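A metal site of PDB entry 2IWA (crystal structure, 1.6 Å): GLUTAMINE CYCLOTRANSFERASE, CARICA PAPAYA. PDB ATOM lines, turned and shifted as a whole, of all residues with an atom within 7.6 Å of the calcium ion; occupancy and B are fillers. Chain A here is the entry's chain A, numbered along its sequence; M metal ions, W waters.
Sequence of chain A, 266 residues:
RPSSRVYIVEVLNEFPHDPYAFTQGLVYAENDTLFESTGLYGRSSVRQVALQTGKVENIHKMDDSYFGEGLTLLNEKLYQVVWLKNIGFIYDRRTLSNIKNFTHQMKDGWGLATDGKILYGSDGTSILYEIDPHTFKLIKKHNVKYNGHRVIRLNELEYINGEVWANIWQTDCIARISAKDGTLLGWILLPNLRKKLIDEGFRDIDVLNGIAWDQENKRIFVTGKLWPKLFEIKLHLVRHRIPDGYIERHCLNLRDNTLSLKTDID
The backbone carbonyl oxygen (O) of Glu 156 is in hydrogen-bond range of the backbone NH (N) of Asn 167 (3.0 Å). N of Trp 165 sits at hydrogen-bond distance from O of Glu 158, 2.8 Å away. The backbone NH (N) of Trp 213 sits at hydrogen-bond distance from the side-chain carboxylate (OE1) of Glu 158, 2.9 Å away.
The nearest printed residue that does not touch the calcium ion is Leu 71 (4.6 Å).
The calcium ion is bound by the backbone carbonyl oxygen (O) of Leu 157. The side-chain carboxylate (OE2) of Glu 158 is bound to the calcium ion, 2.3 Å away. The calcium ion is bound by O of Leu 26, 2.3 Å away. O of Ile 211 is bound to the calcium ion, 2.4 Å away. Water W1 is bound to the calcium ion, 2.4 Å away. OE2 of Glu 156 is bound to the calcium ion (2.5 Å). The calcium ion is bound by OE1 of Glu 156, at 2.6 Å. The calcium ion has seven donor atoms within binding distance.
Water W1 bridges the backbone carbonyl oxygen of Leu 71 (2.7 Å) and the backbone carbonyl oxygen of Leu 112 (2.9 Å).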
ATOM      1  N   GLN A  24     -22.514  30.521  -0.434  1.00  0.00           N
ATOM      2  CA  GLN A  24     -23.269  29.277  -0.470  1.00  0.00           C
ATOM      3  C   GLN A  24     -22.898  28.370  -1.631  1.00  0.00           C
ATOM      4  O   GLN A  24     -23.365  27.233  -1.679  1.00  0.00           O
ATOM      5  CB  GLN A  24     -24.810  29.536  -0.503  1.00  0.00           C
ATOM      6  CG  GLN A  24     -25.312  30.428   0.656  1.00  0.00           C
ATOM      7  CD  GLN A  24     -25.535  29.724   2.016  1.00  0.00           C
ATOM      8  OE1 GLN A  24     -25.995  30.359   2.961  1.00  0.00           O
ATOM      9  NE2 GLN A  24     -25.194  28.431   2.132  1.00  0.00           N
ATOM     10  N   GLY A  25     -22.099  28.888  -2.571  1.00  0.00           N
ATOM     11  CA  GLY A  25     -21.670  28.065  -3.708  1.00  0.00           C
ATOM     12  C   GLY A  25     -20.315  28.581  -4.164  1.00  0.00           C
ATOM     13  O   GLY A  25     -20.091  29.798  -4.152  1.00  0.00           O
ATOM     14  N   LEU A  26     -19.413  27.676  -4.532  1.00  0.00           N
ATOM     15  CA  LEU A  26     -18.059  28.064  -4.929  1.00  0.00           C
ATOM     16  C   LEU A  26     -17.559  27.088  -5.973  1.00  0.00           C
ATOM     17  O   LEU A  26     -17.674  25.850  -5.824  1.00  0.00           O
ATOM     18  CB  LEU A  26     -17.132  28.067  -3.701  1.00  0.00           C
ATOM     19  CG  LEU A  26     -15.775  28.753  -3.918  1.00  0.00           C
ATOM     20  CD1 LEU A  26     -15.951  30.277  -3.967  1.00  0.00           C
ATOM     21  CD2 LEU A  26     -14.834  28.402  -2.764  1.00  0.00           C
ATOM     22  N   VAL A  27     -17.024  27.659  -7.063  1.00  0.00           N
ATOM     23  CA  VAL A  27     -16.619  26.918  -8.282  1.00  0.00           C
ATOM     24  C   VAL A  27     -15.270  27.470  -8.704  1.00  0.00           C
ATOM     25  O   VAL A  27     -15.027  28.669  -8.563  1.00  0.00           O
ATOM     26  CB  VAL A  27     -17.653  27.238  -9.403  1.00  0.00           C
ATOM     27  CG1 VAL A  27     -17.105  26.886 -10.816  1.00  0.00           C
ATOM     28  CG2 VAL A  27     -18.992  26.536  -9.111  1.00  0.00           C
ATOM     29  N   TYR A  28     -14.384  26.583  -9.171  1.00  0.00           N
ATOM     30  CA  TYR A  28     -13.153  27.053  -9.859  1.00  0.00           C
ATOM     31  C   TYR A  28     -13.345  26.750 -11.340  1.00  0.00           C
ATOM     32  O   TYR A  28     -13.680  25.598 -11.698  1.00  0.00           O
ATOM     33  CB  TYR A  28     -11.915  26.294  -9.335  1.00  0.00           C
ATOM     34  CG  TYR A  28     -10.632  26.766 -10.037  1.00  0.00           C
ATOM     35  CD1 TYR A  28     -10.226  26.206 -11.248  1.00  0.00           C
ATOM     36  CD2 TYR A  28      -9.854  27.790  -9.488  1.00  0.00           C
ATOM     37  CE1 TYR A  28      -9.099  26.669 -11.908  1.00  0.00           C
ATOM     38  CE2 TYR A  28      -8.708  28.273 -10.168  1.00  0.00           C
ATOM     39  CZ  TYR A  28      -8.350  27.680 -11.365  1.00  0.00           C
ATOM     40  OH  TYR A  28      -7.245  28.131 -12.043  1.00  0.00           O
ATOM     41  N   PHE A  35     -16.202  31.143  -9.587  1.00  0.00           N
ATOM     42  CA  PHE A  35     -17.611  31.585  -9.566  1.00  0.00           C
ATOM     43  C   PHE A  35     -18.148  31.321  -8.173  1.00  0.00           C
ATOM     44  O   PHE A  35     -17.786  30.328  -7.516  1.00  0.00           O
ATOM     45  CB  PHE A  35     -18.470  30.929 -10.668  1.00  0.00           C
ATOM     46  CG  PHE A  35     -18.108  31.405 -12.050  1.00  0.00           C
ATOM     47  CD1 PHE A  35     -17.201  30.709 -12.822  1.00  0.00           C
ATOM     48  CD2 PHE A  35     -18.696  32.556 -12.561  1.00  0.00           C
ATOM     49  CE1 PHE A  35     -16.816  31.157 -14.127  1.00  0.00           C
ATOM     50  CE2 PHE A  35     -18.342  33.037 -13.869  1.00  0.00           C
ATOM     51  CZ  PHE A  35     -17.421  32.330 -14.649  1.00  0.00           C
ATOM     52  N   GLY A  70     -26.292  26.620  -3.420  1.00  0.00           N
ATOM     53  CA  GLY A  70     -25.167  26.006  -4.118  1.00  0.00           C
ATOM     54  C   GLY A  70     -25.056  26.352  -5.586  1.00  0.00           C
ATOM     55  O   GLY A  70     -26.009  26.848  -6.202  1.00  0.00           O
ATOM     56  N   LEU A  71     -23.868  26.094  -6.131  1.00  0.00           N
ATOM     57  CA  LEU A  71     -23.543  26.508  -7.512  1.00  0.00           C
ATOM     58  C   LEU A  71     -22.526  25.519  -8.049  1.00  0.00           C
ATOM     59  O   LEU A  71     -21.581  25.146  -7.356  1.00  0.00           O
ATOM     60  CB  LEU A  71     -22.848  27.876  -7.440  1.00  0.00           C
ATOM     61  CG  LEU A  71     -22.569  28.573  -8.794  1.00  0.00           C
ATOM     62  CD1 LEU A  71     -23.882  29.075  -9.459  1.00  0.00           C
ATOM     63  CD2 LEU A  71     -21.589  29.716  -8.579  1.00  0.00           C
ATOM     64  N   THR A  72     -22.709  25.126  -9.318  1.00  0.00           N
ATOM     65  CA  THR A  72     -21.704  24.352 -10.031  1.00  0.00           C
ATOM     66  C   THR A  72     -21.633  24.740 -11.481  1.00  0.00           C
ATOM     67  O   THR A  72     -22.505  25.423 -11.965  1.00  0.00           O
ATOM     68  CB  THR A  72     -21.914  22.817  -9.812  1.00  0.00           C
ATOM     69  OG1 THR A  72     -20.736  22.121 -10.236  1.00  0.00           O
ATOM     70  CG2 THR A  72     -23.119  22.278 -10.623  1.00  0.00           C
ATOM     71  N   LEU A 112     -24.516  21.993  -4.857  1.00  0.00           N
ATOM     72  CA  LEU A 112     -24.416  21.364  -6.164  1.00  0.00           C
ATOM     73  C   LEU A 112     -22.960  21.083  -6.500  1.00  0.00           C
ATOM     74  O   LEU A 112     -22.081  21.868  -6.163  1.00  0.00           O
ATOM     75  CB  LEU A 112     -24.946  22.303  -7.256  1.00  0.00           C
ATOM     76  CG  LEU A 112     -26.470  22.510  -7.237  1.00  0.00           C
ATOM     77  CD1 LEU A 112     -26.801  23.576  -8.299  1.00  0.00           C
ATOM     78  CD2 LEU A 112     -27.207  21.175  -7.542  1.00  0.00           C
ATOM     79  N   ALA A 113     -22.744  19.986  -7.245  1.00  0.00           N
ATOM     80  CA  ALA A 113     -21.451  19.690  -7.874  1.00  0.00           C
ATOM     81  C   ALA A 113     -21.692  18.935  -9.158  1.00  0.00           C
ATOM     82  O   ALA A 113     -22.839  18.707  -9.550  1.00  0.00           O
ATOM     83  CB  ALA A 113     -20.609  18.855  -6.893  1.00  0.00           C
ATOM     84  N   GLU A 156     -22.371  22.796   0.971  1.00  0.00           N
ATOM     85  CA  GLU A 156     -21.702  23.112  -0.326  1.00  0.00           C
ATOM     86  C   GLU A 156     -20.900  21.904  -0.788  1.00  0.00           C
ATOM     87  O   GLU A 156     -20.268  21.206   0.037  1.00  0.00           O
ATOM     88  CB  GLU A 156     -20.765  24.320  -0.157  1.00  0.00           C
ATOM     89  CG  GLU A 156     -20.645  25.250  -1.432  1.00  0.00           C
ATOM     90  CD  GLU A 156     -19.701  24.751  -2.514  1.00  0.00           C
ATOM     91  OE1 GLU A 156     -18.626  24.149  -2.216  1.00  0.00           O
ATOM     92  OE2 GLU A 156     -20.011  24.998  -3.723  1.00  0.00           O
ATOM     93  N   LEU A 157     -20.953  21.613  -2.082  1.00  0.00           N
ATOM     94  CA  LEU A 157     -20.339  20.390  -2.617  1.00  0.00           C
ATOM     95  C   LEU A 157     -19.224  20.729  -3.573  1.00  0.00           C
ATOM     96  O   LEU A 157     -19.162  21.828  -4.184  1.00  0.00           O
ATOM     97  CB  LEU A 157     -21.384  19.591  -3.419  1.00  0.00           C
ATOM     98  CG  LEU A 157     -22.613  19.169  -2.628  1.00  0.00           C
ATOM     99  CD1 LEU A 157     -23.533  18.358  -3.541  1.00  0.00           C
ATOM    100  CD2 LEU A 157     -22.262  18.326  -1.369  1.00  0.00           C
ATOM    101  N   GLU A 158     -18.332  19.745  -3.751  1.00  0.00           N
ATOM    102  CA  GLU A 158     -17.348  19.828  -4.848  1.00  0.00           C
ATOM    103  C   GLU A 158     -16.936  18.437  -5.239  1.00  0.00           C
ATOM    104  O   GLU A 158     -16.601  17.624  -4.382  1.00  0.00           O
ATOM    105  CB  GLU A 158     -16.103  20.611  -4.385  1.00  0.00           C
ATOM    106  CG  GLU A 158     -15.141  20.970  -5.500  1.00  0.00           C
ATOM    107  CD  GLU A 158     -15.659  22.040  -6.473  1.00  0.00           C
ATOM    108  OE1 GLU A 158     -14.920  22.359  -7.423  1.00  0.00           O
ATOM    109  OE2 GLU A 158     -16.761  22.587  -6.262  1.00  0.00           O
ATOM    110  N   TYR A 159     -16.950  18.161  -6.538  1.00  0.00           N
ATOM    111  CA  TYR A 159     -16.499  16.862  -7.043  1.00  0.00           C
ATOM    112  C   TYR A 159     -14.985  16.919  -7.259  1.00  0.00           C
ATOM    113  O   TYR A 159     -14.469  17.806  -7.945  1.00  0.00           O
ATOM    114  CB  TYR A 159     -17.195  16.568  -8.363  1.00  0.00           C
ATOM    115  CG  TYR A 159     -16.814  15.248  -8.976  1.00  0.00           C
ATOM    116  CD1 TYR A 159     -17.516  14.092  -8.669  1.00  0.00           C
ATOM    117  CD2 TYR A 159     -15.769  15.186  -9.888  1.00  0.00           C
ATOM    118  CE1 TYR A 159     -17.156  12.844  -9.274  1.00  0.00           C
ATOM    119  CE2 TYR A 159     -15.415  13.963 -10.468  1.00  0.00           C
ATOM    120  CZ  TYR A 159     -16.108  12.819 -10.163  1.00  0.00           C
ATOM    121  OH  TYR A 159     -15.741  11.618 -10.775  1.00  0.00           O
ATOM    122  N   TRP A 165     -17.027  16.059  -2.097  1.00  0.00           N
ATOM    123  CA  TRP A 165     -16.725  16.593  -0.761  1.00  0.00           C
ATOM    124  C   TRP A 165     -17.844  17.523  -0.405  1.00  0.00           C
ATOM    125  O   TRP A 165     -18.323  18.279  -1.252  1.00  0.00           O
ATOM    126  CB  TRP A 165     -15.414  17.378  -0.835  1.00  0.00           C
ATOM    127  CG  TRP A 165     -14.209  16.524  -1.039  1.00  0.00           C
ATOM    128  CD1 TRP A 165     -14.156  15.203  -1.473  1.00  0.00           C
ATOM    129  CD2 TRP A 165     -12.844  16.935  -0.856  1.00  0.00           C
ATOM    130  NE1 TRP A 165     -12.820  14.779  -1.592  1.00  0.00           N
ATOM    131  CE2 TRP A 165     -12.026  15.836  -1.207  1.00  0.00           C
ATOM    132  CE3 TRP A 165     -12.248  18.150  -0.446  1.00  0.00           C
ATOM    133  CZ2 TRP A 165     -10.600  15.919  -1.176  1.00  0.00           C
ATOM    134  CZ3 TRP A 165     -10.858  18.226  -0.417  1.00  0.00           C
ATOM    135  CH2 TRP A 165     -10.051  17.109  -0.760  1.00  0.00           C
ATOM    136  N   ASN A 167     -19.174  20.327   2.657  1.00  0.00           N
ATOM    137  CA  ASN A 167     -19.219  20.986   3.963  1.00  0.00           C
ATOM    138  C   ASN A 167     -20.395  20.412   4.746  1.00  0.00           C
ATOM    139  O   ASN A 167     -21.455  20.094   4.171  1.00  0.00           O
ATOM    140  CB  ASN A 167     -19.486  22.486   3.798  1.00  0.00           C
ATOM    141  CG  ASN A 167     -18.292  23.245   3.260  1.00  0.00           C
ATOM    142  OD1 ASN A 167     -18.253  23.599   2.066  1.00  0.00           O
ATOM    143  ND2 ASN A 167     -17.299  23.495   4.106  1.00  0.00           N
ATOM    144  N   GLY A 210     -17.901  26.410   1.359  1.00  0.00           N
ATOM    145  CA  GLY A 210     -17.419  26.731   0.009  1.00  0.00           C
ATOM    146  C   GLY A 210     -16.128  25.991  -0.261  1.00  0.00           C
ATOM    147  O   GLY A 210     -15.117  26.253   0.431  1.00  0.00           O
ATOM    148  N   ILE A 211     -16.166  25.110  -1.251  1.00  0.00           N
ATOM    149  CA  ILE A 211     -15.034  24.265  -1.633  1.00  0.00           C
ATOM    150  C   ILE A 211     -14.924  24.346  -3.136  1.00  0.00           C
ATOM    151  O   ILE A 211     -15.931  24.172  -3.826  1.00  0.00           O
ATOM    152  CB  ILE A 211     -15.260  22.779  -1.272  1.00  0.00           C
ATOM    153  CG1 ILE A 211     -15.621  22.612   0.201  1.00  0.00           C
ATOM    154  CG2 ILE A 211     -14.002  21.928  -1.631  1.00  0.00           C
ATOM    155  CD1 ILE A 211     -16.302  21.255   0.470  1.00  0.00           C
ATOM    156  N   ALA A 212     -13.715  24.628  -3.643  1.00  0.00           N
ATOM    157  CA  ALA A 212     -13.540  24.679  -5.117  1.00  0.00           C
ATOM    158  C   ALA A 212     -12.245  23.963  -5.462  1.00  0.00           C
ATOM    159  O   ALA A 212     -11.247  24.130  -4.753  1.00  0.00           O
ATOM    160  CB  ALA A 212     -13.493  26.112  -5.602  1.00  0.00           C
ATOM    161  N   TRP A 213     -12.267  23.185  -6.546  1.00  0.00           N
ATOM    162  CA  TRP A 213     -11.123  22.389  -6.978  1.00  0.00           C
ATOM    163  C   TRP A 213     -10.657  22.802  -8.340  1.00  0.00           C
ATOM    164  O   TRP A 213     -11.457  22.871  -9.270  1.00  0.00           O
ATOM    165  CB  TRP A 213     -11.566  20.932  -6.965  1.00  0.00           C
ATOM    166  CG  TRP A 213     -10.650  19.892  -7.619  1.00  0.00           C
ATOM    167  CD1 TRP A 213     -10.971  19.130  -8.713  1.00  0.00           C
ATOM    168  CD2 TRP A 213      -9.340  19.488  -7.213  1.00  0.00           C
ATOM    169  NE1 TRP A 213      -9.924  18.288  -9.027  1.00  0.00           N
ATOM    170  CE2 TRP A 213      -8.920  18.465  -8.107  1.00  0.00           C
ATOM    171  CE3 TRP A 213      -8.499  19.853  -6.160  1.00  0.00           C
ATOM    172  CZ2 TRP A 213      -7.686  17.825  -7.995  1.00  0.00           C
ATOM    173  CZ3 TRP A 213      -7.262  19.203  -6.027  1.00  0.00           C
ATOM    174  CH2 TRP A 213      -6.875  18.210  -6.971  1.00  0.00           C
ATOM    175  N   PHE A 221      -9.396  25.001  -2.781  1.00  0.00           N
ATOM    176  CA  PHE A 221      -9.684  26.308  -2.187  1.00  0.00           C
ATOM    177  C   PHE A 221     -10.902  26.169  -1.300  1.00  0.00           C
ATOM    178  O   PHE A 221     -11.889  25.530  -1.661  1.00  0.00           O
ATOM    179  CB  PHE A 221      -9.971  27.366  -3.262  1.00  0.00           C
ATOM    180  CG  PHE A 221      -8.848  27.545  -4.218  1.00  0.00           C
ATOM    181  CD1 PHE A 221      -7.677  28.198  -3.813  1.00  0.00           C
ATOM    182  CD2 PHE A 221      -8.948  27.037  -5.523  1.00  0.00           C
ATOM    183  CE1 PHE A 221      -6.599  28.368  -4.689  1.00  0.00           C
ATOM    184  CE2 PHE A 221      -7.881  27.223  -6.414  1.00  0.00           C
ATOM    185  CZ  PHE A 221      -6.698  27.888  -5.982  1.00  0.00           C
HETATM  186 CA    CA M   1     -18.069  23.801  -4.761  1.00  0.00          CA
HETATM  187  O   HOH W   1     -19.704  23.427  -6.435  1.00  0.00           O
